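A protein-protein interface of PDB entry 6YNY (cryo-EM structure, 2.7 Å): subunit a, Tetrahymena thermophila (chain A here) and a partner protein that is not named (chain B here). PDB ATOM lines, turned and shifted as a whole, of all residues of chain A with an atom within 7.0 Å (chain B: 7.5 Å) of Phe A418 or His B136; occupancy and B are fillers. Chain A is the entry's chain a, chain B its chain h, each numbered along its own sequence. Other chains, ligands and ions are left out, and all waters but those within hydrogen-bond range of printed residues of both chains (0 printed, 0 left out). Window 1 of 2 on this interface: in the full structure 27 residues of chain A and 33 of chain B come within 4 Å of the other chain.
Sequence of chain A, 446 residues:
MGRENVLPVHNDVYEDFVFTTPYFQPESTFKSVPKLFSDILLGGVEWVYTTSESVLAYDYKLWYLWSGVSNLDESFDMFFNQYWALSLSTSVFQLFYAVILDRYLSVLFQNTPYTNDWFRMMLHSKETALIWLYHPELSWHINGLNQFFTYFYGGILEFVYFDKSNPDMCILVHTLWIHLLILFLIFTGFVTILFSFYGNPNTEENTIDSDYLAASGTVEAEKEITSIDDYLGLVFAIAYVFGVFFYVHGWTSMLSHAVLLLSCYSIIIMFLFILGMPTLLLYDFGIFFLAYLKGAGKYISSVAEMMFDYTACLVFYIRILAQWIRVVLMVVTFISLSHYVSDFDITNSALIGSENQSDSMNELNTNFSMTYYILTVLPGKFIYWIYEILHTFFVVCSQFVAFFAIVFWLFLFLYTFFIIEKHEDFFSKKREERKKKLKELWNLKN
Phe A418 touches just these residues of chain B: Asn B63, Pro B65, Arg B66 and His B136.
Of chain A, only Glu A224 and Phe A418 come within 4 Å of His B136.
Printed residues of chain B within 4 Å of Glu A421: Pro B67 (3.5 Å) and Ser B68 (2.9 Å).
Printed residues of chain A within 4 Å of Asn B61: Glu A222 (3.2 Å) and Glu A224 (3.8 Å).
Printed residues of chain A within 4 Å of Asn B80: Ile A419 (3.9 Å).
Lys A223 touches none of the printed residues of chain B.
Gly B137 touches none of the printed residues of chain A.
The nearest residue of chain A that does not touch His B136 is Ile A419 (5.6 Å).
The nearest printed residue of chain A that does not touch Pro B67 is Phe A417 (5.0 Å).
Of the 20 printed residues of chain B, 9 touch a printed residue of chain A.
Hydrophobic or aromatic side chains of chain B within 4 Å of the printed part of chain A: Pro B65, Pro B67 and His B136.
Of the 10 printed residues of chain A, 8 touch a printed residue of chain B.
Hydrophobic or aromatic side chains of chain A that line the printed part of chain B: Phe A417, Phe A418, Ile A419 and Ile A420.
Among the printed residues, 21 pairs touch across the chains.
Among the printed residues, Asp or Glu carboxylates within 4 Å of a Lys or Arg side-chain nitrogen of the other chain: Glu A222 with Lys B135 and Glu A224 with Lys B135.
OE1 of Glu A222 is in salt-bridge range of NZ of Lys B135 (2.6 Å).
The side-chain carboxylate (OE2) of Glu A224 is in salt-bridge range of the side-chain amino group (NZ) of Lys B135, 3.1 Å away.
The side-chain amide nitrogen of Asn B63 sits at hydrogen-bond distance from the backbone carbonyl oxygen of Thr A416, at 3.2 Å.
The backbone carbonyl oxygen of Phe A418 sits at hydrogen-bond distance from the backbone NH of Arg B66 (3.1 Å).
The side-chain carboxylate (OE2) of Glu A421 sits at hydrogen-bond distance from the backbone NH (N) of Ser B68 (2.9 Å).
O of Trp B57 is in hydrogen-bond range of N of Lys B135 (3.1 Å).
The side-chain amide nitrogen (ND2) of Asn B61 is in hydrogen-bond range of the backbone carbonyl oxygen (O) of Asn B63, at 2.6 Å.
The backbone carbonyl oxygen (O) of His B136 lies close to the side-chain amide oxygen (OD1) of Asn B80, 3.4 Å away.
O of Glu A222 touches CB of Asn B61, at 3.2 Å.
Asn B61 touches Glu A224 (ND2 to CG, 3.8 Å).
CB of Phe A417 touches NH2 of Arg B66, 3.4 Å away.
Phe A417 touches Ser B68 (CE2 to OG, 3.8 Å).
Phe A418 touches Asn B63.
Phe A418 touches Pro B65 (O to CA, 3.2 Å).
O of Arg B66 touches CA of Ile A419, 3.9 Å away.
Ile A420 touches Pro B65.
Ile A420 touches Arg B66.
Pro B67 touches Glu A421.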
ATOM      1  N   GLU A 222     -29.030  19.407 -17.612  1.00  0.00           N
ATOM      2  CA  GLU A 222     -27.614  19.305 -17.930  1.00  0.00           C
ATOM      3  C   GLU A 222     -27.343  19.434 -19.421  1.00  0.00           C
ATOM      4  O   GLU A 222     -26.189  19.637 -19.810  1.00  0.00           O
ATOM      5  CB  GLU A 222     -27.060  17.980 -17.415  1.00  0.00           C
ATOM      6  CG  GLU A 222     -27.199  17.800 -15.922  1.00  0.00           C
ATOM      7  CD  GLU A 222     -26.386  18.806 -15.132  1.00  0.00           C
ATOM      8  OE1 GLU A 222     -25.412  19.353 -15.689  1.00  0.00           O
ATOM      9  OE2 GLU A 222     -26.719  19.053 -13.956  1.00  0.00           O
ATOM     10  N   LYS A 223     -28.368  19.309 -20.264  1.00  0.00           N
ATOM     11  CA  LYS A 223     -28.191  19.594 -21.682  1.00  0.00           C
ATOM     12  C   LYS A 223     -27.968  21.076 -21.938  1.00  0.00           C
ATOM     13  O   LYS A 223     -27.529  21.445 -23.031  1.00  0.00           O
ATOM     14  CB  LYS A 223     -29.397  19.105 -22.481  1.00  0.00           C
ATOM     15  CG  LYS A 223     -29.605  17.598 -22.476  1.00  0.00           C
ATOM     16  CD  LYS A 223     -28.406  16.827 -23.010  1.00  0.00           C
ATOM     17  CE  LYS A 223     -28.121  17.131 -24.468  1.00  0.00           C
ATOM     18  NZ  LYS A 223     -26.877  16.465 -24.913  1.00  0.00           N
ATOM     19  N   GLU A 224     -28.265  21.926 -20.957  1.00  0.00           N
ATOM     20  CA  GLU A 224     -27.960  23.353 -21.025  1.00  0.00           C
ATOM     21  C   GLU A 224     -28.746  24.043 -22.135  1.00  0.00           C
ATOM     22  O   GLU A 224     -28.186  24.708 -23.007  1.00  0.00           O
ATOM     23  CB  GLU A 224     -26.460  23.575 -21.198  1.00  0.00           C
ATOM     24  CG  GLU A 224     -25.618  22.942 -20.111  1.00  0.00           C
ATOM     25  CD  GLU A 224     -25.925  23.486 -18.733  1.00  0.00           C
ATOM     26  OE1 GLU A 224     -26.612  24.524 -18.636  1.00  0.00           O
ATOM     27  OE2 GLU A 224     -25.479  22.872 -17.743  1.00  0.00           O
ATOM     28  N   ILE A 225     -30.063  23.869 -22.101  1.00  0.00           N
ATOM     29  CA  ILE A 225     -30.935  24.631 -22.987  1.00  0.00           C
ATOM     30  C   ILE A 225     -31.156  26.029 -22.428  1.00  0.00           C
ATOM     31  O   ILE A 225     -30.770  27.034 -23.036  1.00  0.00           O
ATOM     32  CB  ILE A 225     -32.269  23.889 -23.183  1.00  0.00           C
ATOM     33  CG1 ILE A 225     -32.023  22.450 -23.634  1.00  0.00           C
ATOM     34  CG2 ILE A 225     -33.139  24.609 -24.185  1.00  0.00           C
ATOM     35  CD1 ILE A 225     -31.195  22.324 -24.886  1.00  0.00           C
ATOM     36  N   THR A 416     -24.844  30.214 -28.631  1.00  0.00           N
ATOM     37  CA  THR A 416     -24.478  30.298 -27.227  1.00  0.00           C
ATOM     38  C   THR A 416     -23.383  29.287 -26.932  1.00  0.00           C
ATOM     39  O   THR A 416     -23.180  28.324 -27.675  1.00  0.00           O
ATOM     40  CB  THR A 416     -25.673  30.043 -26.305  1.00  0.00           C
ATOM     41  OG1 THR A 416     -26.110  28.687 -26.442  1.00  0.00           O
ATOM     42  CG2 THR A 416     -26.818  30.974 -26.637  1.00  0.00           C
ATOM     43  N   PHE A 417     -22.675  29.516 -25.833  1.00  0.00           N
ATOM     44  CA  PHE A 417     -21.583  28.643 -25.433  1.00  0.00           C
ATOM     45  C   PHE A 417     -21.265  28.903 -23.968  1.00  0.00           C
ATOM     46  O   PHE A 417     -21.861  29.770 -23.325  1.00  0.00           O
ATOM     47  CB  PHE A 417     -20.353  28.865 -26.313  1.00  0.00           C
ATOM     48  CG  PHE A 417     -19.476  29.984 -25.852  1.00  0.00           C
ATOM     49  CD1 PHE A 417     -19.944  31.280 -25.818  1.00  0.00           C
ATOM     50  CD2 PHE A 417     -18.177  29.739 -25.458  1.00  0.00           C
ATOM     51  CE1 PHE A 417     -19.139  32.304 -25.391  1.00  0.00           C
ATOM     52  CE2 PHE A 417     -17.370  30.762 -25.033  1.00  0.00           C
ATOM     53  CZ  PHE A 417     -17.851  32.045 -25.000  1.00  0.00           C
ATOM     54  N   PHE A 418     -20.317  28.133 -23.445  1.00  0.00           N
ATOM     55  CA  PHE A 418     -19.809  28.292 -22.093  1.00  0.00           C
ATOM     56  C   PHE A 418     -18.304  28.499 -22.148  1.00  0.00           C
ATOM     57  O   PHE A 418     -17.609  27.852 -22.936  1.00  0.00           O
ATOM     58  CB  PHE A 418     -20.132  27.073 -21.232  1.00  0.00           C
ATOM     59  CG  PHE A 418     -21.596  26.847 -21.030  1.00  0.00           C
ATOM     60  CD1 PHE A 418     -22.280  27.520 -20.040  1.00  0.00           C
ATOM     61  CD2 PHE A 418     -22.286  25.955 -21.823  1.00  0.00           C
ATOM     62  CE1 PHE A 418     -23.622  27.312 -19.851  1.00  0.00           C
ATOM     63  CE2 PHE A 418     -23.627  25.746 -21.635  1.00  0.00           C
ATOM     64  CZ  PHE A 418     -24.295  26.426 -20.646  1.00  0.00           C
ATOM     65  N   ILE A 419     -17.805  29.396 -21.316  1.00  0.00           N
ATOM     66  CA  ILE A 419     -16.378  29.683 -21.296  1.00  0.00           C
ATOM     67  C   ILE A 419     -15.650  28.608 -20.503  1.00  0.00           C
ATOM     68  O   ILE A 419     -16.167  28.054 -19.529  1.00  0.00           O
ATOM     69  CB  ILE A 419     -16.103  31.086 -20.719  1.00  0.00           C
ATOM     70  CG1 ILE A 419     -16.563  31.182 -19.265  1.00  0.00           C
ATOM     71  CG2 ILE A 419     -16.797  32.136 -21.549  1.00  0.00           C
ATOM     72  CD1 ILE A 419     -16.090  32.425 -18.570  1.00  0.00           C
ATOM     73  N   ILE A 420     -14.428  28.308 -20.940  1.00  0.00           N
ATOM     74  CA  ILE A 420     -13.558  27.398 -20.209  1.00  0.00           C
ATOM     75  C   ILE A 420     -12.712  28.128 -19.175  1.00  0.00           C
ATOM     76  O   ILE A 420     -12.219  27.495 -18.230  1.00  0.00           O
ATOM     77  CB  ILE A 420     -12.648  26.640 -21.191  1.00  0.00           C
ATOM     78  CG1 ILE A 420     -11.993  25.436 -20.522  1.00  0.00           C
ATOM     79  CG2 ILE A 420     -11.581  27.559 -21.729  1.00  0.00           C
ATOM     80  CD1 ILE A 420     -12.931  24.318 -20.245  1.00  0.00           C
ATOM     81  N   GLU A 421     -12.535  29.436 -19.320  1.00  0.00           N
ATOM     82  CA  GLU A 421     -11.738  30.208 -18.381  1.00  0.00           C
ATOM     83  C   GLU A 421     -12.528  30.478 -17.109  1.00  0.00           C
ATOM     84  O   GLU A 421     -13.757  30.581 -17.124  1.00  0.00           O
ATOM     85  CB  GLU A 421     -11.304  31.539 -18.995  1.00  0.00           C
ATOM     86  CG  GLU A 421     -10.519  31.421 -20.283  1.00  0.00           C
ATOM     87  CD  GLU A 421     -11.400  31.221 -21.501  1.00  0.00           C
ATOM     88  OE1 GLU A 421     -12.638  31.320 -21.368  1.00  0.00           O
ATOM     89  OE2 GLU A 421     -10.854  30.964 -22.592  1.00  0.00           O
ATOM     90  N   TRP B  57     -20.116  16.342 -11.024  1.00  0.00           N
ATOM     91  CA  TRP B  57     -19.649  17.716 -11.113  1.00  0.00           C
ATOM     92  C   TRP B  57     -19.641  18.262 -12.529  1.00  0.00           C
ATOM     93  O   TRP B  57     -19.890  19.453 -12.713  1.00  0.00           O
ATOM     94  CB  TRP B  57     -18.237  17.846 -10.526  1.00  0.00           C
ATOM     95  CG  TRP B  57     -17.232  16.885 -11.059  1.00  0.00           C
ATOM     96  CD1 TRP B  57     -16.423  17.062 -12.138  1.00  0.00           C
ATOM     97  CD2 TRP B  57     -16.909  15.599 -10.524  1.00  0.00           C
ATOM     98  NE1 TRP B  57     -15.622  15.966 -12.314  1.00  0.00           N
ATOM     99  CE2 TRP B  57     -15.901  15.053 -11.335  1.00  0.00           C
ATOM    100  CE3 TRP B  57     -17.377  14.854  -9.441  1.00  0.00           C
ATOM    101  CZ2 TRP B  57     -15.356  13.799 -11.099  1.00  0.00           C
ATOM    102  CZ3 TRP B  57     -16.834  13.614  -9.210  1.00  0.00           C
ATOM    103  CH2 TRP B  57     -15.834  13.098 -10.034  1.00  0.00           C
ATOM    104  N   HIS B  58     -19.371  17.431 -13.530  1.00  0.00           N
ATOM    105  CA  HIS B  58     -19.335  17.867 -14.925  1.00  0.00           C
ATOM    106  C   HIS B  58     -19.959  16.799 -15.807  1.00  0.00           C
ATOM    107  O   HIS B  58     -19.264  16.070 -16.523  1.00  0.00           O
ATOM    108  CB  HIS B  58     -17.905  18.177 -15.361  1.00  0.00           C
ATOM    109  CG  HIS B  58     -17.827  19.048 -16.574  1.00  0.00           C
ATOM    110  ND1 HIS B  58     -18.818  19.081 -17.529  1.00  0.00           N
ATOM    111  CD2 HIS B  58     -16.887  19.933 -16.976  1.00  0.00           C
ATOM    112  CE1 HIS B  58     -18.487  19.941 -18.474  1.00  0.00           C
ATOM    113  NE2 HIS B  58     -17.319  20.472 -18.162  1.00  0.00           N
ATOM    114  N   ASN B  61     -22.239  16.928 -21.806  1.00  0.00           N
ATOM    115  CA  ASN B  61     -23.264  17.558 -22.619  1.00  0.00           C
ATOM    116  C   ASN B  61     -22.633  17.996 -23.932  1.00  0.00           C
ATOM    117  O   ASN B  61     -21.414  18.149 -24.038  1.00  0.00           O
ATOM    118  CB  ASN B  61     -23.912  18.744 -21.891  1.00  0.00           C
ATOM    119  CG  ASN B  61     -22.968  19.909 -21.714  1.00  0.00           C
ATOM    120  OD1 ASN B  61     -21.989  19.830 -20.975  1.00  0.00           O
ATOM    121  ND2 ASN B  61     -23.272  21.012 -22.380  1.00  0.00           N
ATOM    122  N   ASN B  63     -23.010  20.881 -25.881  1.00  0.00           N
ATOM    123  CA  ASN B  63     -22.460  22.235 -25.858  1.00  0.00           C
ATOM    124  C   ASN B  63     -21.453  22.317 -24.716  1.00  0.00           C
ATOM    125  O   ASN B  63     -21.748  22.759 -23.603  1.00  0.00           O
ATOM    126  CB  ASN B  63     -23.567  23.267 -25.706  1.00  0.00           C
ATOM    127  CG  ASN B  63     -23.087  24.676 -25.955  1.00  0.00           C
ATOM    128  OD1 ASN B  63     -21.889  24.948 -25.944  1.00  0.00           O
ATOM    129  ND2 ASN B  63     -24.023  25.583 -26.176  1.00  0.00           N
ATOM    130  N   ALA B  64     -20.264  21.878 -25.000  1.00  0.00           N
ATOM    131  CA  ALA B  64     -19.217  21.837 -23.996  1.00  0.00           C
ATOM    132  C   ALA B  64     -18.458  23.158 -23.943  1.00  0.00           C
ATOM    133  O   ALA B  64     -18.408  23.893 -24.932  1.00  0.00           O
ATOM    134  CB  ALA B  64     -18.245  20.705 -24.295  1.00  0.00           C
ATOM    135  N   PRO B  65     -17.857  23.481 -22.799  1.00  0.00           N
ATOM    136  CA  PRO B  65     -17.078  24.719 -22.704  1.00  0.00           C
ATOM    137  C   PRO B  65     -15.893  24.717 -23.654  1.00  0.00           C
ATOM    138  O   PRO B  65     -15.174  23.725 -23.783  1.00  0.00           O
ATOM    139  CB  PRO B  65     -16.625  24.738 -21.243  1.00  0.00           C
ATOM    140  CG  PRO B  65     -17.580  23.883 -20.536  1.00  0.00           C
ATOM    141  CD  PRO B  65     -17.968  22.814 -21.492  1.00  0.00           C
ATOM    142  N   ARG B  66     -15.692  25.850 -24.317  1.00  0.00           N
ATOM    143  CA  ARG B  66     -14.597  26.029 -25.251  1.00  0.00           C
ATOM    144  C   ARG B  66     -13.899  27.353 -24.980  1.00  0.00           C
ATOM    145  O   ARG B  66     -14.514  28.289 -24.462  1.00  0.00           O
ATOM    146  CB  ARG B  66     -15.091  25.986 -26.705  1.00  0.00           C
ATOM    147  CG  ARG B  66     -16.152  27.004 -27.058  1.00  0.00           C
ATOM    148  CD  ARG B  66     -16.380  27.032 -28.555  1.00  0.00           C
ATOM    149  NE  ARG B  66     -17.240  28.130 -28.982  1.00  0.00           N
ATOM    150  CZ  ARG B  66     -18.556  28.040 -29.145  1.00  0.00           C
ATOM    151  NH1 ARG B  66     -19.188  26.899 -28.922  1.00  0.00           N
ATOM    152  NH2 ARG B  66     -19.240  29.100 -29.540  1.00  0.00           N
ATOM    153  N   PRO B  67     -12.618  27.456 -25.318  1.00  0.00           N
ATOM    154  CA  PRO B  67     -11.844  28.644 -24.953  1.00  0.00           C
ATOM    155  C   PRO B  67     -12.183  29.848 -25.820  1.00  0.00           C
ATOM    156  O   PRO B  67     -12.852  29.754 -26.848  1.00  0.00           O
ATOM    157  CB  PRO B  67     -10.399  28.198 -25.178  1.00  0.00           C
ATOM    158  CG  PRO B  67     -10.494  27.188 -26.236  1.00  0.00           C
ATOM    159  CD  PRO B  67     -11.791  26.469 -26.027  1.00  0.00           C
ATOM    160  N   SER B  68     -11.689  30.998 -25.373  1.00  0.00           N
ATOM    161  CA  SER B  68     -11.857  32.264 -26.066  1.00  0.00           C
ATOM    162  C   SER B  68     -10.498  32.902 -26.296  1.00  0.00           C
ATOM    163  O   SER B  68      -9.610  32.821 -25.442  1.00  0.00           O
ATOM    164  CB  SER B  68     -12.747  33.214 -25.274  1.00  0.00           C
ATOM    165  OG  SER B  68     -14.033  32.659 -25.074  1.00  0.00           O
ATOM    166  N   ARG B  79     -21.637  36.241 -17.199  1.00  0.00           N
ATOM    167  CA  ARG B  79     -21.997  36.656 -15.852  1.00  0.00           C
ATOM    168  C   ARG B  79     -20.971  36.255 -14.804  1.00  0.00           C
ATOM    169  O   ARG B  79     -21.105  36.660 -13.646  1.00  0.00           O
ATOM    170  CB  ARG B  79     -23.359  36.069 -15.467  1.00  0.00           C
ATOM    171  CG  ARG B  79     -23.397  34.555 -15.425  1.00  0.00           C
ATOM    172  CD  ARG B  79     -24.820  34.041 -15.317  1.00  0.00           C
ATOM    173  NE  ARG B  79     -25.449  34.399 -14.052  1.00  0.00           N
ATOM    174  CZ  ARG B  79     -25.450  33.634 -12.964  1.00  0.00           C
ATOM    175  NH1 ARG B  79     -24.854  32.451 -12.964  1.00  0.00           N
ATOM    176  NH2 ARG B  79     -26.053  34.055 -11.866  1.00  0.00           N
ATOM    177  N   ASN B  80     -19.959  35.478 -15.174  1.00  0.00           N
ATOM    178  CA  ASN B  80     -18.962  35.042 -14.208  1.00  0.00           C
ATOM    179  C   ASN B  80     -18.071  36.201 -13.784  1.00  0.00           C
ATOM    180  O   ASN B  80     -17.707  37.059 -14.592  1.00  0.00           O
ATOM    181  CB  ASN B  80     -18.113  33.919 -14.795  1.00  0.00           C
ATOM    182  CG  ASN B  80     -18.913  32.664 -15.060  1.00  0.00           C
ATOM    183  OD1 ASN B  80     -19.157  31.867 -14.156  1.00  0.00           O
ATOM    184  ND2 ASN B  80     -19.322  32.479 -16.304  1.00  0.00           N
ATOM    185  N   GLN B 133     -14.126  21.269 -10.023  1.00  0.00           N
ATOM    186  CA  GLN B 133     -14.255  20.896 -11.423  1.00  0.00           C
ATOM    187  C   GLN B 133     -15.689  21.012 -11.919  1.00  0.00           C
ATOM    188  O   GLN B 133     -16.004  20.506 -13.001  1.00  0.00           O
ATOM    189  CB  GLN B 133     -13.738  19.475 -11.645  1.00  0.00           C
ATOM    190  CG  GLN B 133     -12.351  19.216 -11.094  1.00  0.00           C
ATOM    191  CD  GLN B 133     -11.302  20.132 -11.680  1.00  0.00           C
ATOM    192  OE1 GLN B 133     -11.537  20.811 -12.679  1.00  0.00           O
ATOM    193  NE2 GLN B 133     -10.137  20.168 -11.049  1.00  0.00           N
ATOM    194  N   ILE B 134     -16.567  21.665 -11.155  1.00  0.00           N
ATOM    195  CA  ILE B 134     -17.953  21.781 -11.569  1.00  0.00           C
ATOM    196  C   ILE B 134     -18.041  22.561 -12.881  1.00  0.00           C
ATOM    197  O   ILE B 134     -17.170  23.370 -13.222  1.00  0.00           O
ATOM    198  CB  ILE B 134     -18.797  22.430 -10.460  1.00  0.00           C
ATOM    199  CG1 ILE B 134     -18.978  21.435  -9.313  1.00  0.00           C
ATOM    200  CG2 ILE B 134     -20.149  22.885 -10.985  1.00  0.00           C
ATOM    201  CD1 ILE B 134     -19.786  21.943  -8.154  1.00  0.00           C
ATOM    202  N   LYS B 135     -19.122  22.308 -13.618  1.00  0.00           N
ATOM    203  CA  LYS B 135     -19.268  22.761 -14.995  1.00  0.00           C
ATOM    204  C   LYS B 135     -18.841  24.206 -15.218  1.00  0.00           C
ATOM    205  O   LYS B 135     -17.877  24.480 -15.942  1.00  0.00           O
ATOM    206  CB  LYS B 135     -20.727  22.596 -15.414  1.00  0.00           C
ATOM    207  CG  LYS B 135     -21.008  21.381 -16.241  1.00  0.00           C
ATOM    208  CD  LYS B 135     -22.473  21.307 -16.583  1.00  0.00           C
ATOM    209  CE  LYS B 135     -22.751  20.233 -17.600  1.00  0.00           C
ATOM    210  NZ  LYS B 135     -24.199  20.075 -17.827  1.00  0.00           N
ATOM    211  N   HIS B 136     -19.547  25.143 -14.596  1.00  0.00           N
ATOM    212  CA  HIS B 136     -19.387  26.560 -14.896  1.00  0.00           C
ATOM    213  C   HIS B 136     -18.989  27.349 -13.657  1.00  0.00           C
ATOM    214  O   HIS B 136     -19.266  28.545 -13.556  1.00  0.00           O
ATOM    215  CB  HIS B 136     -20.673  27.117 -15.500  1.00  0.00           C
ATOM    216  CG  HIS B 136     -21.316  26.200 -16.490  1.00  0.00           C
ATOM    217  ND1 HIS B 136     -22.645  25.842 -16.419  1.00  0.00           N
ATOM    218  CD2 HIS B 136     -20.812  25.558 -17.570  1.00  0.00           C
ATOM    219  CE1 HIS B 136     -22.930  25.021 -17.412  1.00  0.00           C
ATOM    220  NE2 HIS B 136     -21.836  24.832 -18.125  1.00  0.00           N
ATOM    221  N   GLY B 137     -18.329  26.688 -12.714  1.00  0.00           N
ATOM    222  CA  GLY B 137     -17.904  27.330 -11.492  1.00  0.00           C
ATOM    223  C   GLY B 137     -18.763  26.950 -10.308  1.00  0.00           C
ATOM    224  O   GLY B 137     -19.874  27.463 -10.148  1.00  0.00           O
ATOM    225  N   GLY B 138     -18.257  26.042  -9.472  1.00  0.00           N
ATOM    226  CA  GLY B 138     -18.982  25.662  -8.279  1.00  0.00           C
ATOM    227  C   GLY B 138     -19.017  26.743  -7.226  1.00  0.00           C
ATOM    228  O   GLY B 138     -19.932  26.762  -6.397  1.00  0.00           O
ATOM    229  N   GLU B 139     -18.044  27.651  -7.245  1.00  0.00           N
ATOM    230  CA  GLU B 139     -18.005  28.723  -6.260  1.00  0.00           C
ATOM    231  C   GLU B 139     -19.220  29.627  -6.405  1.00  0.00           C
ATOM    232  O   GLU B 139     -19.925  29.905  -5.429  1.00  0.00           O
ATOM    233  CB  GLU B 139     -16.711  29.521  -6.405  1.00  0.00           C
ATOM    234  CG  GLU B 139     -15.440  28.739  -6.116  1.00  0.00           C
ATOM    235  CD  GLU B 139     -15.028  27.817  -7.240  1.00  0.00           C
ATOM    236  OE1 GLU B 139     -15.794  27.680  -8.214  1.00  0.00           O
ATOM    237  OE2 GLU B 139     -13.932  27.227  -7.150  1.00  0.00           O
ATOM    238  N   ARG B 140     -19.478  30.098  -7.625  1.00  0.00           N
ATOM    239  CA  ARG B 140     -20.649  30.928  -7.873  1.00  0.00           C
ATOM    240  C   ARG B 140     -21.933  30.163  -7.605  1.00  0.00           C
ATOM    241  O   ARG B 140     -22.922  30.746  -7.151  1.00  0.00           O
ATOM    242  CB  ARG B 140     -20.620  31.432  -9.314  1.00  0.00           C
ATOM    243  CG  ARG B 140     -21.812  32.256  -9.734  1.00  0.00           C
ATOM    244  CD  ARG B 140     -21.940  33.522  -8.929  1.00  0.00           C
ATOM    245  NE  ARG B 140     -23.020  34.364  -9.429  1.00  0.00           N
ATOM    246  CZ  ARG B 140     -22.888  35.240 -10.418  1.00  0.00           C
ATOM    247  NH1 ARG B 140     -21.722  35.400 -11.023  1.00  0.00           N
ATOM    248  NH2 ARG B 140     -23.930  35.958 -10.807  1.00  0.00           N
ATOM    249  N   ARG B 141     -21.937  28.860  -7.881  1.00  0.00           N
ATOM    250  CA  ARG B 141     -23.142  28.062  -7.708  1.00  0.00           C
ATOM    251  C   ARG B 141     -23.537  27.974  -6.240  1.00  0.00           C
ATOM    252  O   ARG B 141     -24.696  28.211  -5.883  1.00  0.00           O
ATOM    253  CB  ARG B 141     -22.919  26.671  -8.293  1.00  0.00           C
ATOM    254  CG  ARG B 141     -24.119  25.770  -8.225  1.00  0.00           C
ATOM    255  CD  ARG B 141     -23.872  24.458  -8.926  1.00  0.00           C
ATOM    256  NE  ARG B 141     -23.701  24.619 -10.363  1.00  0.00           N
ATOM    257  CZ  ARG B 141     -23.792  23.620 -11.231  1.00  0.00           C
ATOM    258  NH1 ARG B 141     -24.054  22.395 -10.811  1.00  0.00           N
ATOM    259  NH2 ARG B 141     -23.627  23.846 -12.523  1.00  0.00           N
